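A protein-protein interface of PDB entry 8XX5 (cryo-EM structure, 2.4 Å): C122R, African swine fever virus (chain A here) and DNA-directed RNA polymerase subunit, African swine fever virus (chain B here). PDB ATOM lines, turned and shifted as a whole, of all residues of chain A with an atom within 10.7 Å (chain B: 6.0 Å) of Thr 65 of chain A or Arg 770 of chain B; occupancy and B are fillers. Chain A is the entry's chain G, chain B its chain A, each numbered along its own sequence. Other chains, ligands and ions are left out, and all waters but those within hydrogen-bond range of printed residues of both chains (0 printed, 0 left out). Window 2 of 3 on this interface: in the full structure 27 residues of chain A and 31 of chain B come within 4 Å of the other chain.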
ATOM      1  N   PHE A  56      12.533 -22.357  20.319  1.00  0.00           N
ATOM      2  CA  PHE A  56      11.918 -21.367  21.196  1.00  0.00           C
ATOM      3  C   PHE A  56      10.690 -21.930  21.900  1.00  0.00           C
ATOM      4  O   PHE A  56      10.494 -21.699  23.097  1.00  0.00           O
ATOM      5  CB  PHE A  56      11.549 -20.115  20.400  1.00  0.00           C
ATOM      6  CG  PHE A  56      10.827 -19.081  21.208  1.00  0.00           C
ATOM      7  CD1 PHE A  56      11.528 -18.206  22.019  1.00  0.00           C
ATOM      8  CD2 PHE A  56       9.446 -18.989  21.166  1.00  0.00           C
ATOM      9  CE1 PHE A  56      10.865 -17.258  22.768  1.00  0.00           C
ATOM     10  CE2 PHE A  56       8.781 -18.044  21.914  1.00  0.00           C
ATOM     11  CZ  PHE A  56       9.491 -17.178  22.715  1.00  0.00           C
ATOM     12  N   ASN A  59      11.779 -24.206  24.596  1.00  0.00           N
ATOM     13  CA  ASN A  59      12.340 -23.457  25.712  1.00  0.00           C
ATOM     14  C   ASN A  59      11.368 -22.458  26.322  1.00  0.00           C
ATOM     15  O   ASN A  59      11.686 -21.870  27.359  1.00  0.00           O
ATOM     16  CB  ASN A  59      13.602 -22.713  25.264  1.00  0.00           C
ATOM     17  CG  ASN A  59      14.788 -23.632  25.083  1.00  0.00           C
ATOM     18  OD1 ASN A  59      14.988 -24.565  25.858  1.00  0.00           O
ATOM     19  ND2 ASN A  59      15.587 -23.368  24.058  1.00  0.00           N
ATOM     20  N   ALA A  60      10.205 -22.250  25.706  1.00  0.00           N
ATOM     21  CA  ALA A  60       9.265 -21.252  26.207  1.00  0.00           C
ATOM     22  C   ALA A  60       8.826 -21.472  27.651  1.00  0.00           C
ATOM     23  O   ALA A  60       8.755 -20.479  28.396  1.00  0.00           O
ATOM     24  CB  ALA A  60       8.047 -21.182  25.278  1.00  0.00           C
ATOM     25  N   PRO A  61       8.501 -22.689  28.108  1.00  0.00           N
ATOM     26  CA  PRO A  61       8.100 -22.838  29.518  1.00  0.00           C
ATOM     27  C   PRO A  61       9.169 -22.416  30.509  1.00  0.00           C
ATOM     28  O   PRO A  61       8.834 -21.944  31.600  1.00  0.00           O
ATOM     29  CB  PRO A  61       7.788 -24.335  29.635  1.00  0.00           C
ATOM     30  CG  PRO A  61       7.485 -24.767  28.262  1.00  0.00           C
ATOM     31  CD  PRO A  61       8.368 -23.962  27.377  1.00  0.00           C
ATOM     32  N   PHE A  62      10.446 -22.577  30.168  1.00  0.00           N
ATOM     33  CA  PHE A  62      11.535 -22.251  31.079  1.00  0.00           C
ATOM     34  C   PHE A  62      11.988 -20.802  30.980  1.00  0.00           C
ATOM     35  O   PHE A  62      12.766 -20.354  31.828  1.00  0.00           O
ATOM     36  CB  PHE A  62      12.727 -23.178  30.825  1.00  0.00           C
ATOM     37  CG  PHE A  62      12.366 -24.634  30.811  1.00  0.00           C
ATOM     38  CD1 PHE A  62      12.384 -25.375  31.979  1.00  0.00           C
ATOM     39  CD2 PHE A  62      12.001 -25.261  29.632  1.00  0.00           C
ATOM     40  CE1 PHE A  62      12.048 -26.713  31.972  1.00  0.00           C
ATOM     41  CE2 PHE A  62      11.664 -26.597  29.619  1.00  0.00           C
ATOM     42  CZ  PHE A  62      11.688 -27.323  30.789  1.00  0.00           C
ATOM     43  N   ASP A  63      11.523 -20.063  29.983  1.00  0.00           N
ATOM     44  CA  ASP A  63      11.895 -18.663  29.847  1.00  0.00           C
ATOM     45  C   ASP A  63      11.112 -17.829  30.854  1.00  0.00           C
ATOM     46  O   ASP A  63       9.877 -17.810  30.796  1.00  0.00           O
ATOM     47  CB  ASP A  63      11.620 -18.181  28.429  1.00  0.00           C
ATOM     48  CG  ASP A  63      12.355 -16.902  28.092  1.00  0.00           C
ATOM     49  OD1 ASP A  63      13.164 -16.437  28.918  1.00  0.00           O
ATOM     50  OD2 ASP A  63      12.124 -16.360  26.993  1.00  0.00           O
ATOM     51  N   PRO A  64      11.774 -17.135  31.782  1.00  0.00           N
ATOM     52  CA  PRO A  64      11.032 -16.349  32.779  1.00  0.00           C
ATOM     53  C   PRO A  64      10.425 -15.072  32.227  1.00  0.00           C
ATOM     54  O   PRO A  64       9.641 -14.428  32.936  1.00  0.00           O
ATOM     55  CB  PRO A  64      12.095 -16.042  33.839  1.00  0.00           C
ATOM     56  CG  PRO A  64      13.375 -16.047  33.085  1.00  0.00           C
ATOM     57  CD  PRO A  64      13.228 -17.091  32.013  1.00  0.00           C
ATOM     58  N   THR A  65      10.754 -14.685  30.998  1.00  0.00           N
ATOM     59  CA  THR A  65      10.227 -13.473  30.393  1.00  0.00           C
ATOM     60  C   THR A  65       8.995 -13.724  29.537  1.00  0.00           C
ATOM     61  O   THR A  65       8.477 -12.782  28.933  1.00  0.00           O
ATOM     62  CB  THR A  65      11.308 -12.790  29.550  1.00  0.00           C
ATOM     63  OG1 THR A  65      11.557 -13.561  28.371  1.00  0.00           O
ATOM     64  CG2 THR A  65      12.593 -12.667  30.344  1.00  0.00           C
ATOM     65  N   ASN A  66       8.516 -14.960  29.472  1.00  0.00           N
ATOM     66  CA  ASN A  66       7.351 -15.296  28.671  1.00  0.00           C
ATOM     67  C   ASN A  66       6.072 -15.069  29.464  1.00  0.00           C
ATOM     68  O   ASN A  66       6.030 -15.250  30.683  1.00  0.00           O
ATOM     69  CB  ASN A  66       7.423 -16.749  28.203  1.00  0.00           C
ATOM     70  CG  ASN A  66       7.891 -16.877  26.770  1.00  0.00           C
ATOM     71  OD1 ASN A  66       8.955 -17.428  26.501  1.00  0.00           O
ATOM     72  ND2 ASN A  66       7.093 -16.368  25.840  1.00  0.00           N
ATOM     73  N   CYS A  67       5.021 -14.666  28.753  1.00  0.00           N
ATOM     74  CA  CYS A  67       3.735 -14.414  29.388  1.00  0.00           C
ATOM     75  C   CYS A  67       3.125 -15.706  29.914  1.00  0.00           C
ATOM     76  O   CYS A  67       3.156 -16.745  29.249  1.00  0.00           O
ATOM     77  CB  CYS A  67       2.775 -13.753  28.401  1.00  0.00           C
ATOM     78  SG  CYS A  67       1.392 -12.885  29.171  1.00  0.00           S
ATOM     79  N   GLN A  68       2.563 -15.634  31.115  1.00  0.00           N
ATOM     80  CA  GLN A  68       1.857 -16.748  31.725  1.00  0.00           C
ATOM     81  C   GLN A  68       0.398 -16.372  31.935  1.00  0.00           C
ATOM     82  O   GLN A  68       0.068 -15.206  32.169  1.00  0.00           O
ATOM     83  CB  GLN A  68       2.487 -17.148  33.063  1.00  0.00           C
ATOM     84  CG  GLN A  68       3.993 -17.027  33.091  1.00  0.00           C
ATOM     85  CD  GLN A  68       4.681 -18.292  32.636  1.00  0.00           C
ATOM     86  OE1 GLN A  68       4.344 -19.388  33.078  1.00  0.00           O
ATOM     87  NE2 GLN A  68       5.651 -18.149  31.743  1.00  0.00           N
ATOM     88  N   ILE A  69      -0.476 -17.372  31.849  1.00  0.00           N
ATOM     89  CA  ILE A  69      -1.904 -17.175  32.048  1.00  0.00           C
ATOM     90  C   ILE A  69      -2.394 -18.157  33.100  1.00  0.00           C
ATOM     91  O   ILE A  69      -1.802 -19.213  33.326  1.00  0.00           O
ATOM     92  CB  ILE A  69      -2.713 -17.338  30.744  1.00  0.00           C
ATOM     93  CG1 ILE A  69      -2.618 -18.775  30.231  1.00  0.00           C
ATOM     94  CG2 ILE A  69      -2.233 -16.356  29.693  1.00  0.00           C
ATOM     95  CD1 ILE A  69      -3.524 -19.054  29.062  1.00  0.00           C
ATOM     96  N   LEU A  81       0.000 -21.594  32.726  1.00  0.00           N
ATOM     97  CA  LEU A  81       0.604 -22.061  31.490  1.00  0.00           C
ATOM     98  C   LEU A  81       1.345 -20.908  30.835  1.00  0.00           C
ATOM     99  O   LEU A  81       0.953 -19.747  30.965  1.00  0.00           O
ATOM    100  CB  LEU A  81      -0.446 -22.621  30.521  1.00  0.00           C
ATOM    101  CG  LEU A  81      -1.017 -24.003  30.828  1.00  0.00           C
ATOM    102  CD1 LEU A  81      -2.197 -24.295  29.924  1.00  0.00           C
ATOM    103  CD2 LEU A  81       0.051 -25.065  30.667  1.00  0.00           C
ATOM    104  N   THR A  82       2.421 -21.238  30.130  1.00  0.00           N
ATOM    105  CA  THR A  82       3.135 -20.247  29.340  1.00  0.00           C
ATOM    106  C   THR A  82       2.374 -19.988  28.046  1.00  0.00           C
ATOM    107  O   THR A  82       1.956 -20.927  27.362  1.00  0.00           O
ATOM    108  CB  THR A  82       4.555 -20.722  29.039  1.00  0.00           C
ATOM    109  OG1 THR A  82       5.249 -20.959  30.270  1.00  0.00           O
ATOM    110  CG2 THR A  82       5.307 -19.679  28.234  1.00  0.00           C
ATOM    111  N   GLN A  83       2.191 -18.715  27.713  1.00  0.00           N
ATOM    112  CA  GLN A  83       1.394 -18.307  26.564  1.00  0.00           C
ATOM    113  C   GLN A  83       2.312 -17.699  25.512  1.00  0.00           C
ATOM    114  O   GLN A  83       3.056 -16.757  25.804  1.00  0.00           O
ATOM    115  CB  GLN A  83       0.314 -17.313  26.986  1.00  0.00           C
ATOM    116  CG  GLN A  83      -0.279 -16.513  25.849  1.00  0.00           C
ATOM    117  CD  GLN A  83      -1.566 -15.830  26.249  1.00  0.00           C
ATOM    118  OE1 GLN A  83      -2.629 -16.446  26.260  1.00  0.00           O
ATOM    119  NE2 GLN A  83      -1.477 -14.547  26.580  1.00  0.00           N
ATOM    120  N   ILE A  84       2.253 -18.232  24.297  1.00  0.00           N
ATOM    121  CA  ILE A  84       3.077 -17.773  23.187  1.00  0.00           C
ATOM    122  C   ILE A  84       2.162 -17.237  22.096  1.00  0.00           C
ATOM    123  O   ILE A  84       1.016 -17.672  21.953  1.00  0.00           O
ATOM    124  CB  ILE A  84       3.979 -18.899  22.633  1.00  0.00           C
ATOM    125  CG1 ILE A  84       4.560 -19.739  23.767  1.00  0.00           C
ATOM    126  CG2 ILE A  84       5.107 -18.333  21.799  1.00  0.00           C
ATOM    127  CD1 ILE A  84       5.032 -21.096  23.310  1.00  0.00           C
ATOM    128  N   CYS A  85       2.676 -16.283  21.323  1.00  0.00           N
ATOM    129  CA  CYS A  85       1.938 -15.705  20.200  1.00  0.00           C
ATOM    130  C   CYS A  85       2.929 -15.481  19.062  1.00  0.00           C
ATOM    131  O   CYS A  85       3.618 -14.459  19.025  1.00  0.00           O
ATOM    132  CB  CYS A  85       1.247 -14.410  20.602  1.00  0.00           C
ATOM    133  SG  CYS A  85       0.035 -13.824  19.410  1.00  0.00           S
ATOM    134  N   ARG A  97       6.136 -26.847  31.191  1.00  0.00           N
ATOM    135  CA  ARG A  97       7.431 -27.482  31.390  1.00  0.00           C
ATOM    136  C   ARG A  97       7.322 -28.998  31.459  1.00  0.00           C
ATOM    137  O   ARG A  97       8.330 -29.689  31.273  1.00  0.00           O
ATOM    138  CB  ARG A  97       8.093 -26.946  32.658  1.00  0.00           C
ATOM    139  CG  ARG A  97       7.156 -26.805  33.842  1.00  0.00           C
ATOM    140  CD  ARG A  97       7.938 -26.478  35.097  1.00  0.00           C
ATOM    141  NE  ARG A  97       8.912 -25.420  34.856  1.00  0.00           N
ATOM    142  CZ  ARG A  97       9.975 -25.192  35.614  1.00  0.00           C
ATOM    143  NH1 ARG A  97      10.247 -25.945  36.667  1.00  0.00           N
ATOM    144  NH2 ARG A  97      10.787 -24.184  35.306  1.00  0.00           N
ATOM    145  N   GLN B 763       6.077  -0.749  19.010  1.00  0.00           N
ATOM    146  CA  GLN B 763       6.551  -1.991  18.427  1.00  0.00           C
ATOM    147  C   GLN B 763       7.386  -2.779  19.434  1.00  0.00           C
ATOM    148  O   GLN B 763       8.077  -2.196  20.273  1.00  0.00           O
ATOM    149  CB  GLN B 763       7.380  -1.709  17.181  1.00  0.00           C
ATOM    150  CG  GLN B 763       6.587  -1.070  16.056  1.00  0.00           C
ATOM    151  CD  GLN B 763       5.276  -1.780  15.804  1.00  0.00           C
ATOM    152  OE1 GLN B 763       5.254  -2.915  15.333  1.00  0.00           O
ATOM    153  NE2 GLN B 763       4.172  -1.113  16.117  1.00  0.00           N
ATOM    154  N   PRO B 764       7.334  -4.108  19.374  1.00  0.00           N
ATOM    155  CA  PRO B 764       8.175  -4.942  20.259  1.00  0.00           C
ATOM    156  C   PRO B 764       9.629  -5.003  19.795  1.00  0.00           C
ATOM    157  O   PRO B 764      10.095  -5.952  19.167  1.00  0.00           O
ATOM    158  CB  PRO B 764       7.487  -6.306  20.187  1.00  0.00           C
ATOM    159  CG  PRO B 764       6.829  -6.323  18.857  1.00  0.00           C
ATOM    160  CD  PRO B 764       6.397  -4.916  18.575  1.00  0.00           C
ATOM    161  N   GLN B 765      10.379  -3.951  20.119  1.00  0.00           N
ATOM    162  CA  GLN B 765      11.765  -3.831  19.689  1.00  0.00           C
ATOM    163  C   GLN B 765      12.772  -4.206  20.767  1.00  0.00           C
ATOM    164  O   GLN B 765      13.957  -4.346  20.455  1.00  0.00           O
ATOM    165  CB  GLN B 765      12.049  -2.402  19.210  1.00  0.00           C
ATOM    166  CG  GLN B 765      10.907  -1.776  18.431  1.00  0.00           C
ATOM    167  CD  GLN B 765      11.038  -1.986  16.935  1.00  0.00           C
ATOM    168  OE1 GLN B 765      11.080  -3.119  16.458  1.00  0.00           O
ATOM    169  NE2 GLN B 765      11.098  -0.891  16.187  1.00  0.00           N
ATOM    170  N   PHE B 766      12.340  -4.366  22.020  1.00  0.00           N
ATOM    171  CA  PHE B 766      13.273  -4.748  23.075  1.00  0.00           C
ATOM    172  C   PHE B 766      13.828  -6.145  22.831  1.00  0.00           C
ATOM    173  O   PHE B 766      15.042  -6.368  22.908  1.00  0.00           O
ATOM    174  CB  PHE B 766      12.587  -4.671  24.437  1.00  0.00           C
ATOM    175  CG  PHE B 766      13.444  -5.139  25.570  1.00  0.00           C
ATOM    176  CD1 PHE B 766      14.523  -4.385  25.994  1.00  0.00           C
ATOM    177  CD2 PHE B 766      13.176  -6.333  26.211  1.00  0.00           C
ATOM    178  CE1 PHE B 766      15.316  -4.815  27.036  1.00  0.00           C
ATOM    179  CE2 PHE B 766      13.966  -6.768  27.251  1.00  0.00           C
ATOM    180  CZ  PHE B 766      15.038  -6.008  27.664  1.00  0.00           C
ATOM    181  N   SER B 767      12.951  -7.099  22.540  1.00  0.00           N
ATOM    182  CA  SER B 767      13.346  -8.438  22.134  1.00  0.00           C
ATOM    183  C   SER B 767      12.301  -8.949  21.155  1.00  0.00           C
ATOM    184  O   SER B 767      11.442  -8.195  20.688  1.00  0.00           O
ATOM    185  CB  SER B 767      13.490  -9.373  23.340  1.00  0.00           C
ATOM    186  OG  SER B 767      13.997  -8.692  24.469  1.00  0.00           O
ATOM    187  N   PHE B 768      12.372 -10.237  20.845  1.00  0.00           N
ATOM    188  CA  PHE B 768      11.330 -10.877  20.056  1.00  0.00           C
ATOM    189  C   PHE B 768      10.062 -10.959  20.896  1.00  0.00           C
ATOM    190  O   PHE B 768       9.985 -11.753  21.837  1.00  0.00           O
ATOM    191  CB  PHE B 768      11.790 -12.260  19.605  1.00  0.00           C
ATOM    192  CG  PHE B 768      10.675 -13.140  19.130  1.00  0.00           C
ATOM    193  CD1 PHE B 768       9.849 -12.738  18.096  1.00  0.00           C
ATOM    194  CD2 PHE B 768      10.456 -14.372  19.717  1.00  0.00           C
ATOM    195  CE1 PHE B 768       8.824 -13.545  17.663  1.00  0.00           C
ATOM    196  CE2 PHE B 768       9.436 -15.185  19.285  1.00  0.00           C
ATOM    197  CZ  PHE B 768       8.615 -14.769  18.257  1.00  0.00           C
ATOM    198  N   GLY B 769       9.073 -10.130  20.572  1.00  0.00           N
ATOM    199  CA  GLY B 769       7.819 -10.121  21.296  1.00  0.00           C
ATOM    200  C   GLY B 769       7.795  -9.295  22.563  1.00  0.00           C
ATOM    201  O   GLY B 769       6.801  -9.350  23.294  1.00  0.00           O
ATOM    202  N   ARG B 770       8.846  -8.531  22.849  1.00  0.00           N
ATOM    203  CA  ARG B 770       8.922  -7.710  24.051  1.00  0.00           C
ATOM    204  C   ARG B 770       9.043  -6.245  23.666  1.00  0.00           C
ATOM    205  O   ARG B 770       9.860  -5.890  22.810  1.00  0.00           O
ATOM    206  CB  ARG B 770      10.112  -8.108  24.928  1.00  0.00           C
ATOM    207  CG  ARG B 770      10.009  -9.480  25.551  1.00  0.00           C
ATOM    208  CD  ARG B 770      11.097  -9.687  26.586  1.00  0.00           C
ATOM    209  NE  ARG B 770      10.756  -9.077  27.864  1.00  0.00           N
ATOM    210  CZ  ARG B 770      11.579  -9.004  28.901  1.00  0.00           C
ATOM    211  NH1 ARG B 770      12.809  -9.486  28.841  1.00  0.00           N
ATOM    212  NH2 ARG B 770      11.158  -8.433  30.023  1.00  0.00           N
ATOM    213  N   THR B 771       8.242  -5.395  24.306  1.00  0.00           N
ATOM    214  CA  THR B 771       8.348  -3.956  24.110  1.00  0.00           C
ATOM    215  C   THR B 771       9.307  -3.304  25.095  1.00  0.00           C
ATOM    216  O   THR B 771       9.972  -2.324  24.743  1.00  0.00           O
ATOM    217  CB  THR B 771       6.972  -3.295  24.235  1.00  0.00           C
ATOM    218  OG1 THR B 771       6.341  -3.724  25.446  1.00  0.00           O
ATOM    219  CG2 THR B 771       6.093  -3.672  23.058  1.00  0.00           C
ATOM    220  N   LEU B 772       9.391  -3.824  26.315  1.00  0.00           N
ATOM    221  CA  LEU B 772      10.273  -3.285  27.338  1.00  0.00           C
ATOM    222  C   LEU B 772      10.707  -4.423  28.249  1.00  0.00           C
ATOM    223  O   LEU B 772      10.122  -5.508  28.242  1.00  0.00           O
ATOM    224  CB  LEU B 772       9.588  -2.180  28.152  1.00  0.00           C
ATOM    225  CG  LEU B 772       9.604  -0.747  27.617  1.00  0.00           C
ATOM    226  CD1 LEU B 772       8.917   0.187  28.597  1.00  0.00           C
ATOM    227  CD2 LEU B 772      11.022  -0.282  27.338  1.00  0.00           C
ATOM    228  N   VAL B 773      11.750  -4.163  29.039  1.00  0.00           N
ATOM    229  CA  VAL B 773      12.170  -5.125  30.049  1.00  0.00           C
ATOM    230  C   VAL B 773      11.129  -5.261  31.152  1.00  0.00           C
ATOM    231  O   VAL B 773      11.152  -6.239  31.907  1.00  0.00           O
ATOM    232  CB  VAL B 773      13.541  -4.726  30.630  1.00  0.00           C
ATOM    233  CG1 VAL B 773      13.386  -3.661  31.707  1.00  0.00           C
ATOM    234  CG2 VAL B 773      14.270  -5.945  31.175  1.00  0.00           C
ATOM    235  N   TYR B 774      10.206  -4.308  31.256  1.00  0.00           N
ATOM    236  CA  TYR B 774       9.199  -4.295  32.306  1.00  0.00           C
ATOM    237  C   TYR B 774       7.970  -5.125  31.973  1.00  0.00           C
ATOM    238  O   TYR B 774       7.118  -5.318  32.846  1.00  0.00           O
ATOM    239  CB  TYR B 774       8.772  -2.855  32.599  1.00  0.00           C
ATOM    240  CG  TYR B 774       9.901  -1.987  33.090  1.00  0.00           C
ATOM    241  CD1 TYR B 774      10.598  -2.313  34.243  1.00  0.00           C
ATOM    242  CD2 TYR B 774      10.276  -0.847  32.397  1.00  0.00           C
ATOM    243  CE1 TYR B 774      11.633  -1.527  34.695  1.00  0.00           C
ATOM    244  CE2 TYR B 774      11.310  -0.054  32.842  1.00  0.00           C
ATOM    245  CZ  TYR B 774      11.984  -0.397  33.992  1.00  0.00           C
ATOM    246  OH  TYR B 774      13.017   0.390  34.438  1.00  0.00           O
ATOM    247  N   TYR B 775       7.856  -5.622  30.746  1.00  0.00           N
ATOM    248  CA  TYR B 775       6.688  -6.382  30.348  1.00  0.00           C
ATOM    249  C   TYR B 775       7.100  -7.743  29.802  1.00  0.00           C
ATOM    250  O   TYR B 775       8.168  -7.876  29.198  1.00  0.00           O
ATOM    251  CB  TYR B 775       5.878  -5.627  29.287  1.00  0.00           C
ATOM    252  CG  TYR B 775       5.311  -4.322  29.789  1.00  0.00           C
ATOM    253  CD1 TYR B 775       4.225  -4.302  30.652  1.00  0.00           C
ATOM    254  CD2 TYR B 775       5.866  -3.110  29.407  1.00  0.00           C
ATOM    255  CE1 TYR B 775       3.705  -3.114  31.115  1.00  0.00           C
ATOM    256  CE2 TYR B 775       5.353  -1.916  29.865  1.00  0.00           C
ATOM    257  CZ  TYR B 775       4.273  -1.924  30.719  1.00  0.00           C
ATOM    258  OH  TYR B 775       3.756  -0.737  31.179  1.00  0.00           O
ATOM    259  N   PRO B 776       6.279  -8.769  30.002  1.00  0.00           N
ATOM    260  CA  PRO B 776       6.647 -10.107  29.535  1.00  0.00           C
ATOM    261  C   PRO B 776       6.551 -10.224  28.024  1.00  0.00           C
ATOM    262  O   PRO B 776       5.933  -9.406  27.341  1.00  0.00           O
ATOM    263  CB  PRO B 776       5.625 -11.015  30.224  1.00  0.00           C
ATOM    264  CG  PRO B 776       4.449 -10.146  30.425  1.00  0.00           C
ATOM    265  CD  PRO B 776       4.984  -8.771  30.701  1.00  0.00           C
ATOM    266  N   ARG B 777       7.191 -11.266  27.509  1.00  0.00           N
ATOM    267  CA  ARG B 777       7.116 -11.564  26.089  1.00  0.00           C
ATOM    268  C   ARG B 777       5.691 -11.942  25.703  1.00  0.00           C
ATOM    269  O   ARG B 777       5.013 -12.678  26.422  1.00  0.00           O
ATOM    270  CB  ARG B 777       8.077 -12.697  25.742  1.00  0.00           C
ATOM    271  CG  ARG B 777       8.378 -12.831  24.272  1.00  0.00           C
ATOM    272  CD  ARG B 777       9.396 -13.927  24.032  1.00  0.00           C
ATOM    273  NE  ARG B 777      10.756 -13.407  23.999  1.00  0.00           N
ATOM    274  CZ  ARG B 777      11.676 -13.672  24.915  1.00  0.00           C
ATOM    275  NH1 ARG B 777      11.414 -14.447  25.953  1.00  0.00           N
ATOM    276  NH2 ARG B 777      12.888 -13.141  24.789  1.00  0.00           N
ATOM    277  N   PHE B 778       5.241 -11.421  24.560  1.00  0.00           N
ATOM    278  CA  PHE B 778       3.891 -11.660  24.048  1.00  0.00           C
ATOM    279  C   PHE B 778       2.817 -11.211  25.033  1.00  0.00           C
ATOM    280  O   PHE B 778       1.764 -11.841  25.146  1.00  0.00           O
ATOM    281  CB  PHE B 778       3.680 -13.130  23.677  1.00  0.00           C
ATOM    282  CG  PHE B 778       4.788 -13.708  22.860  1.00  0.00           C
ATOM    283  CD1 PHE B 778       5.084 -13.194  21.612  1.00  0.00           C
ATOM    284  CD2 PHE B 778       5.536 -14.766  23.341  1.00  0.00           C
ATOM    285  CE1 PHE B 778       6.105 -13.723  20.858  1.00  0.00           C
ATOM    286  CE2 PHE B 778       6.556 -15.299  22.591  1.00  0.00           C
ATOM    287  CZ  PHE B 778       6.841 -14.778  21.349  1.00  0.00           C
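NH2 of Arg 777 of chain B lies within salt-bridge range of OD2 of Asp 63 of chain A. The backbone carbonyl oxygen of Arg 777 of chain B lies within hydrogen-bond range of the backbone NH of Cys 67 of chain A (3.1 Å). The backbone carbonyl oxygen (O) of Thr 65 of chain A lies within hydrogen-bond range of the backbone NH (N) of Arg 777 of chain B.
Among the printed residues, pairs that only touch across the chains: Phe 56 of chain A with Phe 768 of chain B (3.9 Å), Phe 56 of chain A with Arg 777 of chain B (3.5 Å), Phe 56 of chain A with Phe 778 of chain B (3.5 Å), Thr 65 of chain A with Arg 770 of chain B (3.5 Å), Thr 65 of chain A with Pro 776 of chain B (3.3 Å), Asn 66 of chain A with Arg 777 of chain B (3.8 Å), Asn 66 of chain A with Phe 778 of chain B (3.4 Å), Cys 67 of chain A with Pro 776 of chain B (3.98 Å), Cys 67 of chain A with Phe 778 of chain B (3.9 Å), Ile 84 of chain A with Phe 778 of chain B (3.5 Å) and Cys 85 of chain A with Phe 778 of chain B (3.2 Å).
Of the printed residues of chain B, Asp 63 of chain A touches Arg 777. Thr 65 of chain A touches three residues of chain B. Of the printed residues of chain B, Asn 66 of chain A touches Arg 777 and Phe 778. Leu 81 of chain A touches none of the printed residues of chain B. No residue of chain A comes within 4 Å of Pro 764 of chain B. No residue of chain A comes within 4 Å of Ser 767 of chain B. Arg 770 of chain B touches just one residue of chain A: Thr 65. No residue of chain A comes within 4 Å of Val 773 of chain B. Tyr 774 of chain B touches none of the printed residues of chain A. Printed residues of chain A within 4 Å of Arg 777 of chain B: Phe 56, Asp 63, Thr 65, Asn 66 and Cys 67. Printed residues of chain A within 4 Å of Phe 778 of chain B: Phe 56, Asn 66, Cys 67, Ile 84 and Cys 85. The nearest residue of chain A that does not touch Arg 770 of chain B is Asn 66 of chain A (6.5 Å).
Hydrophobic or aromatic side chains of chain B within 4 Å of the printed part of chain A: Phe 768, Pro 776 and Phe 778. Of the 18 printed residues of chain A, 7 touch a printed residue of chain B.
The side-chain carboxylate of Asp 63 of chain A sits close to the side-chain amide oxygen of Asn 66 of chain A (3.4 Å). O of Cys 67 of chain A lies within hydrogen-bond range of N of Gln 83 of chain A (2.7 Å). The guanidinium group of Arg 770 of chain B is in hydrogen-bond range of the backbone carbonyl oxygen of Val 773 of chain B (2.9 Å). O of Phe 768 of chain B lies within hydrogen-bond range of NE of Arg 777 of chain B (2.8 Å). The backbone carbonyl oxygen of Gly 769 of chain B sits at hydrogen-bond distance from the backbone NH of Phe 778 of chain B (2.9 Å). N of Gln 765 of chain B lies within hydrogen-bond range of O of Arg 770 of chain B (3.4 Å).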
